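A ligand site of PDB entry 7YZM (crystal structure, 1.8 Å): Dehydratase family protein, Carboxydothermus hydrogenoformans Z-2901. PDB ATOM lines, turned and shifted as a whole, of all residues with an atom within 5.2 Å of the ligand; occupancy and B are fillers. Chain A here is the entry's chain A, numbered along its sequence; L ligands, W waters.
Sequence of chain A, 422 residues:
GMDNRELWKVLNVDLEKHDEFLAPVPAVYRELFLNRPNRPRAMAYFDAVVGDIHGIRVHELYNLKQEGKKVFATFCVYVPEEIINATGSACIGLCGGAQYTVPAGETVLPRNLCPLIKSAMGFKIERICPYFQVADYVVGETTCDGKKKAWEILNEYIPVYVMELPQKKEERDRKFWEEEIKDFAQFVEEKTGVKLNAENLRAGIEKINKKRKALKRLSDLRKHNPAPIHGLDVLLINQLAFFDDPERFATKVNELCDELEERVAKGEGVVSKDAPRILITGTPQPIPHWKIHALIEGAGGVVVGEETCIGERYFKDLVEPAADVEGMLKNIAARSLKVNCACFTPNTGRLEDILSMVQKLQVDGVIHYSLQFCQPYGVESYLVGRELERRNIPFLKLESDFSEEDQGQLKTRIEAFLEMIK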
ATOM      1  N   PHE A  75      13.858  -5.690  23.217  1.00  0.00           N
ATOM      2  CA  PHE A  75      14.807  -6.199  24.198  1.00  0.00           C
ATOM      3  C   PHE A  75      15.432  -7.521  23.748  1.00  0.00           C
ATOM      4  O   PHE A  75      16.115  -8.168  24.549  1.00  0.00           O
ATOM      5  CB  PHE A  75      14.122  -6.400  25.549  1.00  0.00           C
ATOM      6  CG  PHE A  75      13.704  -5.120  26.189  1.00  0.00           C
ATOM      7  CD1 PHE A  75      14.575  -4.419  27.003  1.00  0.00           C
ATOM      8  CD2 PHE A  75      12.442  -4.597  25.957  1.00  0.00           C
ATOM      9  CE1 PHE A  75      14.194  -3.238  27.581  1.00  0.00           C
ATOM     10  CE2 PHE A  75      12.062  -3.407  26.539  1.00  0.00           C
ATOM     11  CZ  PHE A  75      12.938  -2.728  27.351  1.00  0.00           C
ATOM     12  N   CYS A  76      15.222  -7.923  22.506  1.00  0.00           N
ATOM     13  CA  CYS A  76      15.685  -9.218  22.033  1.00  0.00           C
ATOM     14  C   CYS A  76      15.939  -9.116  20.536  1.00  0.00           C
ATOM     15  O   CYS A  76      15.192  -8.450  19.820  1.00  0.00           O
ATOM     16  CB  CYS A  76      14.652 -10.297  22.337  1.00  0.00           C
ATOM     17  SG  CYS A  76      15.066 -11.927  21.686  1.00  0.00           S
ATOM     18  N   VAL A  77      16.993  -9.781  20.064  1.00  0.00           N
ATOM     19  CA  VAL A  77      17.296  -9.735  18.643  1.00  0.00           C
ATOM     20  C   VAL A  77      16.270 -10.486  17.808  1.00  0.00           C
ATOM     21  O   VAL A  77      16.286 -10.372  16.580  1.00  0.00           O
ATOM     22  CB  VAL A  77      18.698 -10.308  18.361  1.00  0.00           C
ATOM     23  CG1 VAL A  77      19.729  -9.575  19.182  1.00  0.00           C
ATOM     24  CG2 VAL A  77      18.734 -11.817  18.622  1.00  0.00           C
ATOM     25  N   TYR A  78      15.386 -11.267  18.447  1.00  0.00           N
ATOM     26  CA  TYR A  78      14.386 -12.023  17.708  1.00  0.00           C
ATOM     27  C   TYR A  78      13.272 -11.141  17.160  1.00  0.00           C
ATOM     28  O   TYR A  78      12.590 -11.550  16.224  1.00  0.00           O
ATOM     29  CB  TYR A  78      13.788 -13.124  18.595  1.00  0.00           C
ATOM     30  CG  TYR A  78      14.464 -14.457  18.389  1.00  0.00           C
ATOM     31  CD1 TYR A  78      15.574 -14.833  19.136  1.00  0.00           C
ATOM     32  CD2 TYR A  78      14.015 -15.329  17.415  1.00  0.00           C
ATOM     33  CE1 TYR A  78      16.202 -16.062  18.925  1.00  0.00           C
ATOM     34  CE2 TYR A  78      14.630 -16.548  17.208  1.00  0.00           C
ATOM     35  CZ  TYR A  78      15.719 -16.910  17.953  1.00  0.00           C
ATOM     36  OH  TYR A  78      16.324 -18.133  17.707  1.00  0.00           O
ATOM     37  N   CYS A  95      17.814  -2.836  26.104  1.00  0.00           N
ATOM     38  CA  CYS A  95      18.340  -3.672  27.171  1.00  0.00           C
ATOM     39  C   CYS A  95      19.143  -2.838  28.165  1.00  0.00           C
ATOM     40  O   CYS A  95      20.007  -2.061  27.774  1.00  0.00           O
ATOM     41  CB  CYS A  95      19.218  -4.778  26.583  1.00  0.00           C
ATOM     42  SG  CYS A  95      18.251  -6.033  25.729  1.00  0.00           S
ATOM     43  N   CYS A 114      17.850 -11.171  36.883  1.00  0.00           N
ATOM     44  CA  CYS A 114      18.880 -10.650  36.005  1.00  0.00           C
ATOM     45  C   CYS A 114      18.931  -9.125  36.073  1.00  0.00           C
ATOM     46  O   CYS A 114      17.887  -8.477  35.956  1.00  0.00           O
ATOM     47  CB  CYS A 114      18.599 -11.066  34.563  1.00  0.00           C
ATOM     48  SG  CYS A 114      19.772 -10.400  33.395  1.00  0.00           S
ATOM     49  N   LEU A 116      19.877  -7.055  33.809  1.00  0.00           N
ATOM     50  CA  LEU A 116      19.405  -6.443  32.580  1.00  0.00           C
ATOM     51  C   LEU A 116      17.931  -6.084  32.707  1.00  0.00           C
ATOM     52  O   LEU A 116      17.519  -4.972  32.361  1.00  0.00           O
ATOM     53  CB  LEU A 116      19.626  -7.391  31.398  1.00  0.00           C
ATOM     54  CG  LEU A 116      19.303  -6.889  29.987  1.00  0.00           C
ATOM     55  CD1 LEU A 116      20.219  -7.594  28.975  1.00  0.00           C
ATOM     56  CD2 LEU A 116      17.852  -7.104  29.632  1.00  0.00           C
ATOM     57  N   ILE A 117      17.140  -7.019  33.240  1.00  0.00           N
ATOM     58  CA  ILE A 117      15.709  -6.820  33.381  1.00  0.00           C
ATOM     59  C   ILE A 117      15.426  -5.768  34.445  1.00  0.00           C
ATOM     60  O   ILE A 117      14.606  -4.867  34.243  1.00  0.00           O
ATOM     61  CB  ILE A 117      15.019  -8.152  33.738  1.00  0.00           C
ATOM     62  CG1 ILE A 117      15.424  -9.248  32.752  1.00  0.00           C
ATOM     63  CG2 ILE A 117      13.510  -7.968  33.800  1.00  0.00           C
ATOM     64  CD1 ILE A 117      14.998 -10.636  33.178  1.00  0.00           C
ATOM     65  N   GLU A 141       9.096 -10.643  24.265  1.00  0.00           N
ATOM     66  CA  GLU A 141       9.273 -11.974  23.719  1.00  0.00           C
ATOM     67  C   GLU A 141       9.264 -12.970  24.863  1.00  0.00           C
ATOM     68  O   GLU A 141       9.713 -12.654  25.974  1.00  0.00           O
ATOM     69  CB  GLU A 141      10.582 -12.029  22.917  1.00  0.00           C
ATOM     70  CG  GLU A 141      11.807 -12.372  23.741  1.00  0.00           C
ATOM     71  CD  GLU A 141      12.392 -11.233  24.562  1.00  0.00           C
ATOM     72  OE1 GLU A 141      11.980 -10.061  24.458  1.00  0.00           O
ATOM     73  OE2 GLU A 141      13.332 -11.529  25.322  1.00  0.00           O
ATOM     74  N   THR A 143      11.149 -15.359  26.043  1.00  0.00           N
ATOM     75  CA  THR A 143      12.450 -16.003  26.154  1.00  0.00           C
ATOM     76  C   THR A 143      12.689 -16.501  27.584  1.00  0.00           C
ATOM     77  O   THR A 143      12.188 -17.569  27.952  1.00  0.00           O
ATOM     78  CB  THR A 143      13.563 -15.038  25.728  1.00  0.00           C
ATOM     79  OG1 THR A 143      13.335 -13.748  26.313  1.00  0.00           O
ATOM     80  CG2 THR A 143      13.582 -14.921  24.206  1.00  0.00           C
ATOM     81  N   CYS A 144      13.456 -15.759  28.378  1.00  0.00           N
ATOM     82  CA  CYS A 144      13.744 -16.211  29.726  1.00  0.00           C
ATOM     83  C   CYS A 144      12.561 -15.947  30.648  1.00  0.00           C
ATOM     84  O   CYS A 144      11.651 -15.173  30.325  1.00  0.00           O
ATOM     85  CB  CYS A 144      15.007 -15.537  30.260  1.00  0.00           C
ATOM     86  SG  CYS A 144      14.807 -13.745  30.353  1.00  0.00           S
ATOM     87  N   LYS A 147      12.156 -12.057  31.858  1.00  0.00           N
ATOM     88  CA  LYS A 147      11.561 -11.166  30.867  1.00  0.00           C
ATOM     89  C   LYS A 147      10.094 -11.490  30.637  1.00  0.00           C
ATOM     90  O   LYS A 147       9.241 -10.608  30.611  1.00  0.00           O
ATOM     91  CB  LYS A 147      12.311 -11.282  29.537  1.00  0.00           C
ATOM     92  CG  LYS A 147      13.569 -10.456  29.440  1.00  0.00           C
ATOM     93  CD  LYS A 147      14.295 -10.791  28.158  1.00  0.00           C
ATOM     94  CE  LYS A 147      15.231  -9.685  27.753  1.00  0.00           C
ATOM     95  NZ  LYS A 147      15.986 -10.041  26.522  1.00  0.00           N
ATOM     96  N   THR A 283      26.084 -13.875  27.671  1.00  0.00           N
ATOM     97  CA  THR A 283      24.956 -12.951  27.616  1.00  0.00           C
ATOM     98  C   THR A 283      25.358 -11.651  26.946  1.00  0.00           C
ATOM     99  O   THR A 283      26.549 -11.324  26.852  1.00  0.00           O
ATOM    100  CB  THR A 283      24.432 -12.680  29.035  1.00  0.00           C
ATOM    101  OG1 THR A 283      25.524 -12.325  29.900  1.00  0.00           O
ATOM    102  CG2 THR A 283      23.732 -13.884  29.599  1.00  0.00           C
ATOM    103  N   PRO A 284      24.392 -10.887  26.439  1.00  0.00           N
ATOM    104  CA  PRO A 284      24.719  -9.568  25.884  1.00  0.00           C
ATOM    105  C   PRO A 284      25.230  -8.640  26.976  1.00  0.00           C
ATOM    106  O   PRO A 284      24.869  -8.759  28.152  1.00  0.00           O
ATOM    107  CB  PRO A 284      23.388  -9.080  25.307  1.00  0.00           C
ATOM    108  CG  PRO A 284      22.324  -9.855  26.015  1.00  0.00           C
ATOM    109  CD  PRO A 284      22.944 -11.190  26.376  1.00  0.00           C
ATOM    110  N   CYS A 309      24.527 -11.647  21.913  1.00  0.00           N
ATOM    111  CA  CYS A 309      23.556 -10.897  21.130  1.00  0.00           C
ATOM    112  C   CYS A 309      23.876  -9.407  21.010  1.00  0.00           C
ATOM    113  O   CYS A 309      23.162  -8.702  20.292  1.00  0.00           O
ATOM    114  CB  CYS A 309      22.168 -11.087  21.720  1.00  0.00           C
ATOM    115  SG  CYS A 309      21.462 -12.606  21.092  1.00  0.00           S
ATOM    116  N   ARG A 313      25.850 -12.922  17.565  1.00  0.00           N
ATOM    117  CA  ARG A 313      24.491 -13.440  17.418  1.00  0.00           C
ATOM    118  C   ARG A 313      23.557 -12.403  16.802  1.00  0.00           C
ATOM    119  O   ARG A 313      22.526 -12.764  16.221  1.00  0.00           O
ATOM    120  CB  ARG A 313      23.924 -13.898  18.760  1.00  0.00           C
ATOM    121  CG  ARG A 313      24.644 -15.139  19.328  1.00  0.00           C
ATOM    122  CD  ARG A 313      23.799 -15.911  20.332  1.00  0.00           C
ATOM    123  NE  ARG A 313      23.444 -15.105  21.502  1.00  0.00           N
ATOM    124  CZ  ARG A 313      24.062 -15.166  22.678  1.00  0.00           C
ATOM    125  NH1 ARG A 313      25.065 -16.010  22.873  1.00  0.00           N
ATOM    126  NH2 ARG A 313      23.651 -14.370  23.664  1.00  0.00           N
ATOM    127  N   VAL A 339      19.331 -17.740  15.239  1.00  0.00           N
ATOM    128  CA  VAL A 339      20.016 -17.249  16.440  1.00  0.00           C
ATOM    129  C   VAL A 339      19.986 -18.334  17.513  1.00  0.00           C
ATOM    130  O   VAL A 339      18.911 -18.793  17.924  1.00  0.00           O
ATOM    131  CB  VAL A 339      19.371 -15.943  16.938  1.00  0.00           C
ATOM    132  CG1 VAL A 339      19.955 -15.567  18.279  1.00  0.00           C
ATOM    133  CG2 VAL A 339      19.585 -14.816  15.898  1.00  0.00           C
ATOM    134  N   CYS A 341      20.261 -18.918  20.823  1.00  0.00           N
ATOM    135  CA  CYS A 341      20.130 -18.453  22.205  1.00  0.00           C
ATOM    136  C   CYS A 341      19.892 -19.624  23.138  1.00  0.00           C
ATOM    137  O   CYS A 341      19.223 -20.597  22.761  1.00  0.00           O
ATOM    138  CB  CYS A 341      18.961 -17.471  22.324  1.00  0.00           C
ATOM    139  SG  CYS A 341      18.435 -17.125  24.029  1.00  0.00           S
ATOM    140  N   CYS A 343      17.904 -19.942  25.408  1.00  0.00           N
ATOM    141  CA  CYS A 343      16.504 -20.220  25.723  1.00  0.00           C
ATOM    142  C   CYS A 343      15.947 -21.372  24.896  1.00  0.00           C
ATOM    143  O   CYS A 343      14.869 -21.874  25.223  1.00  0.00           O
ATOM    144  CB  CYS A 343      15.662 -18.948  25.541  1.00  0.00           C
ATOM    145  SG  CYS A 343      16.004 -17.666  26.801  1.00  0.00           S
ATOM    146  N   LEU A 371      25.478 -12.798  33.042  1.00  0.00           N
ATOM    147  CA  LEU A 371      25.007 -11.960  34.137  1.00  0.00           C
ATOM    148  C   LEU A 371      24.464 -12.801  35.288  1.00  0.00           C
ATOM    149  O   LEU A 371      23.863 -13.857  35.081  1.00  0.00           O
ATOM    150  CB  LEU A 371      23.933 -10.984  33.638  1.00  0.00           C
ATOM    151  CG  LEU A 371      24.375  -9.981  32.575  1.00  0.00           C
ATOM    152  CD1 LEU A 371      23.178  -9.215  32.016  1.00  0.00           C
ATOM    153  CD2 LEU A 371      25.405  -9.019  33.157  1.00  0.00           C
ATOM    154  N   PHE A 373      22.187 -14.417  37.899  1.00  0.00           N
ATOM    155  CA  PHE A 373      20.805 -14.885  37.885  1.00  0.00           C
ATOM    156  C   PHE A 373      20.255 -15.080  36.482  1.00  0.00           C
ATOM    157  O   PHE A 373      19.045 -15.273  36.310  1.00  0.00           O
ATOM    158  CB  PHE A 373      19.883 -13.954  38.696  1.00  0.00           C
ATOM    159  CG  PHE A 373      20.429 -13.625  40.059  1.00  0.00           C
ATOM    160  CD1 PHE A 373      20.605 -14.626  41.014  1.00  0.00           C
ATOM    161  CD2 PHE A 373      20.782 -12.329  40.387  1.00  0.00           C
ATOM    162  CE1 PHE A 373      21.126 -14.326  42.261  1.00  0.00           C
ATOM    163  CE2 PHE A 373      21.303 -12.029  41.634  1.00  0.00           C
ATOM    164  CZ  PHE A 373      21.478 -13.034  42.572  1.00  0.00           C
ATOM    165  N   CYS A 374      21.102 -15.046  35.441  1.00  0.00           N
ATOM    166  CA  CYS A 374      20.684 -15.494  34.127  1.00  0.00           C
ATOM    167  C   CYS A 374      20.766 -17.005  34.121  1.00  0.00           C
ATOM    168  O   CYS A 374      21.851 -17.580  34.000  1.00  0.00           O
ATOM    169  CB  CYS A 374      21.548 -14.912  33.021  1.00  0.00           C
ATOM    170  SG  CYS A 374      21.120 -15.664  31.433  1.00  0.00           S
ATOM    171  N   GLN A 375      19.624 -17.671  34.244  1.00  0.00           N
ATOM    172  CA  GLN A 375      19.635 -19.116  34.371  1.00  0.00           C
ATOM    173  C   GLN A 375      19.856 -19.800  33.032  1.00  0.00           C
ATOM    174  O   GLN A 375      20.601 -20.787  32.969  1.00  0.00           O
ATOM    175  CB  GLN A 375      18.344 -19.572  35.070  1.00  0.00           C
ATOM    176  CG  GLN A 375      18.362 -19.182  36.548  1.00  0.00           C
ATOM    177  CD  GLN A 375      17.019 -19.268  37.251  1.00  0.00           C
ATOM    178  OE1 GLN A 375      15.975 -19.428  36.625  1.00  0.00           O
ATOM    179  NE2 GLN A 375      17.038 -19.143  38.576  1.00  0.00           N
ATOM    180  N   PRO A 376      19.280 -19.319  31.923  1.00  0.00           N
ATOM    181  CA  PRO A 376      19.556 -19.973  30.632  1.00  0.00           C
ATOM    182  C   PRO A 376      21.046 -20.115  30.321  1.00  0.00           C
ATOM    183  O   PRO A 376      21.509 -21.214  30.013  1.00  0.00           O
ATOM    184  CB  PRO A 376      18.824 -19.090  29.619  1.00  0.00           C
ATOM    185  CG  PRO A 376      17.616 -18.552  30.418  1.00  0.00           C
ATOM    186  CD  PRO A 376      18.183 -18.325  31.818  1.00  0.00           C
ATOM    187  N   TYR A 377      21.813 -19.026  30.415  1.00  0.00           N
ATOM    188  CA  TYR A 377      23.239 -19.086  30.106  1.00  0.00           C
ATOM    189  C   TYR A 377      24.056 -19.620  31.279  1.00  0.00           C
ATOM    190  O   TYR A 377      25.086 -20.258  31.060  1.00  0.00           O
ATOM    191  CB  TYR A 377      23.730 -17.692  29.673  1.00  0.00           C
ATOM    192  CG  TYR A 377      23.242 -17.372  28.281  1.00  0.00           C
ATOM    193  CD1 TYR A 377      23.982 -17.746  27.157  1.00  0.00           C
ATOM    194  CD2 TYR A 377      22.012 -16.755  28.075  1.00  0.00           C
ATOM    195  CE1 TYR A 377      23.530 -17.496  25.882  1.00  0.00           C
ATOM    196  CE2 TYR A 377      21.546 -16.499  26.787  1.00  0.00           C
ATOM    197  CZ  TYR A 377      22.324 -16.869  25.701  1.00  0.00           C
ATOM    198  OH  TYR A 377      21.886 -16.630  24.421  1.00  0.00           O
HETATM  199  S1  LIG L   1      18.210 -13.666  32.246  1.00  0.00           S
HETATM  200  S2  LIG L   1      18.382 -14.290  28.754  1.00  0.00           S
HETATM  201  S3  LIG L   1      17.422 -10.928  30.167  1.00  0.00           S
HETATM  202  S4  LIG L   1      20.780 -12.005  30.142  1.00  0.00           S
HETATM  203  S5  LIG L   1      18.598 -10.857  23.072  1.00  0.00           S
HETATM  204  S6  LIG L   1      20.428 -13.743  24.649  1.00  0.00           S
HETATM  205  S7  LIG L   1      16.804 -13.479  25.009  1.00  0.00           S
HETATM  206  S8  LIG L   1      18.026 -14.163  21.666  1.00  0.00           S
HETATM  207  S9  LIG L   1      18.981 -10.909  26.852  1.00  0.00           S
HETATM  208 FE1  LIG L   1      18.991 -12.033  28.817  1.00  0.00          FE
HETATM  209 FE2  LIG L   1      19.039 -11.621  31.489  1.00  0.00          FE
HETATM  210 FE3  LIG L   1      19.670 -14.002  30.540  1.00  0.00          FE
HETATM  211 FE4  LIG L   1      17.148 -13.150  30.394  1.00  0.00          FE
HETATM  212 FE5  LIG L   1      18.448 -14.684  23.960  1.00  0.00          FE
HETATM  213 FE6  LIG L   1      17.052 -12.548  22.903  1.00  0.00          FE
HETATM  214 FE7  LIG L   1      19.709 -12.836  22.593  1.00  0.00          FE
HETATM  215 FE8  LIG L   1      18.736 -12.227  25.053  1.00  0.00          FE
HETATM  216  O   HOH W   1      15.314 -14.616  33.699  1.00  0.00           O
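The side-chain sulfur (SG) of Cys 374 is bound to an iron atom (FE3) of the ligand (2.4 Å). NZ of Lys 147 lies close to S9 of the ligand, 3.1 Å away. The side-chain sulfur (SG) of Cys 76 is bound to an iron atom (FE6) of the ligand (2.4 Å). An iron atom (FE2) of the ligand is bound by the side-chain sulfur (SG) of Cys 114 (2.4 Å). FE4 of the ligand is bound by SG of Cys 144 (2.4 Å). OH of Tyr 377 lies close to S6 of the ligand, 3.2 Å away. A sulfur (S7) of the ligand lies close to the side-chain hydroxyl of Thr 143, at 3.7 Å. SG of Cys 309 is bound to FE7 of the ligand, at 2.3 Å. The backbone NH (N) of Val 77 sits close to a sulfur (S5) of the ligand. FE5 of the ligand is bound by SG of Cys 341, at 2.4 Å. NH2 of Arg 313 lies close to S6 of the ligand.
The backbone NH (N) of Leu 371 sits at hydrogen-bond distance from the side-chain hydroxyl (OG1) of Thr 283. SG of Cys 76 sits close to N of Tyr 78 (3.3 Å). The side-chain sulfur of Cys 341 sits close to the backbone NH of Cys 343 (3.2 Å). N of Tyr 377 sits close to SG of Cys 374 (3.6 Å). The side-chain sulfur (SG) of Cys 95 lies within hydrogen-bond range of the backbone carbonyl oxygen (O) of Phe 75 (3.2 Å). The side-chain sulfur (SG) of Cys 309 sits close to the guanidinium group (NE) of Arg 313, at 3.2 Å. The side-chain carboxylate of Glu 141 is in salt-bridge range of the side-chain amino group of Lys 147 (3.3 Å). OH of Tyr 377 sits close to SG of Cys 341 (3.5 Å).
Phe 75 touches the ligand. CD1 of Tyr 78 touches S8 of the ligand, 3.6 Å away. Leu 116 touches the ligand. Ile 117 touches the ligand (CG1 to S3, 3.7 Å). Glu 141 touches the ligand (OE2 to S7, 3.99 Å). CG2 of Thr 283 touches S4 of the ligand, 3.5 Å away. Pro 284 touches the ligand (CG to S9, 3.6 Å). Within 4 Å of the ligand: Phe 75, Cys 76, Val 77, Tyr 78, Cys 114, Leu 116, Ile 117, Glu 141, Thr 143, Cys 144, Lys 147, Thr 283, Pro 284, Cys 309, Arg 313, Cys 341, Cys 374 and Tyr 377. Along chain A the residues within 4 Å of the ligand span positions 75 to 377.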
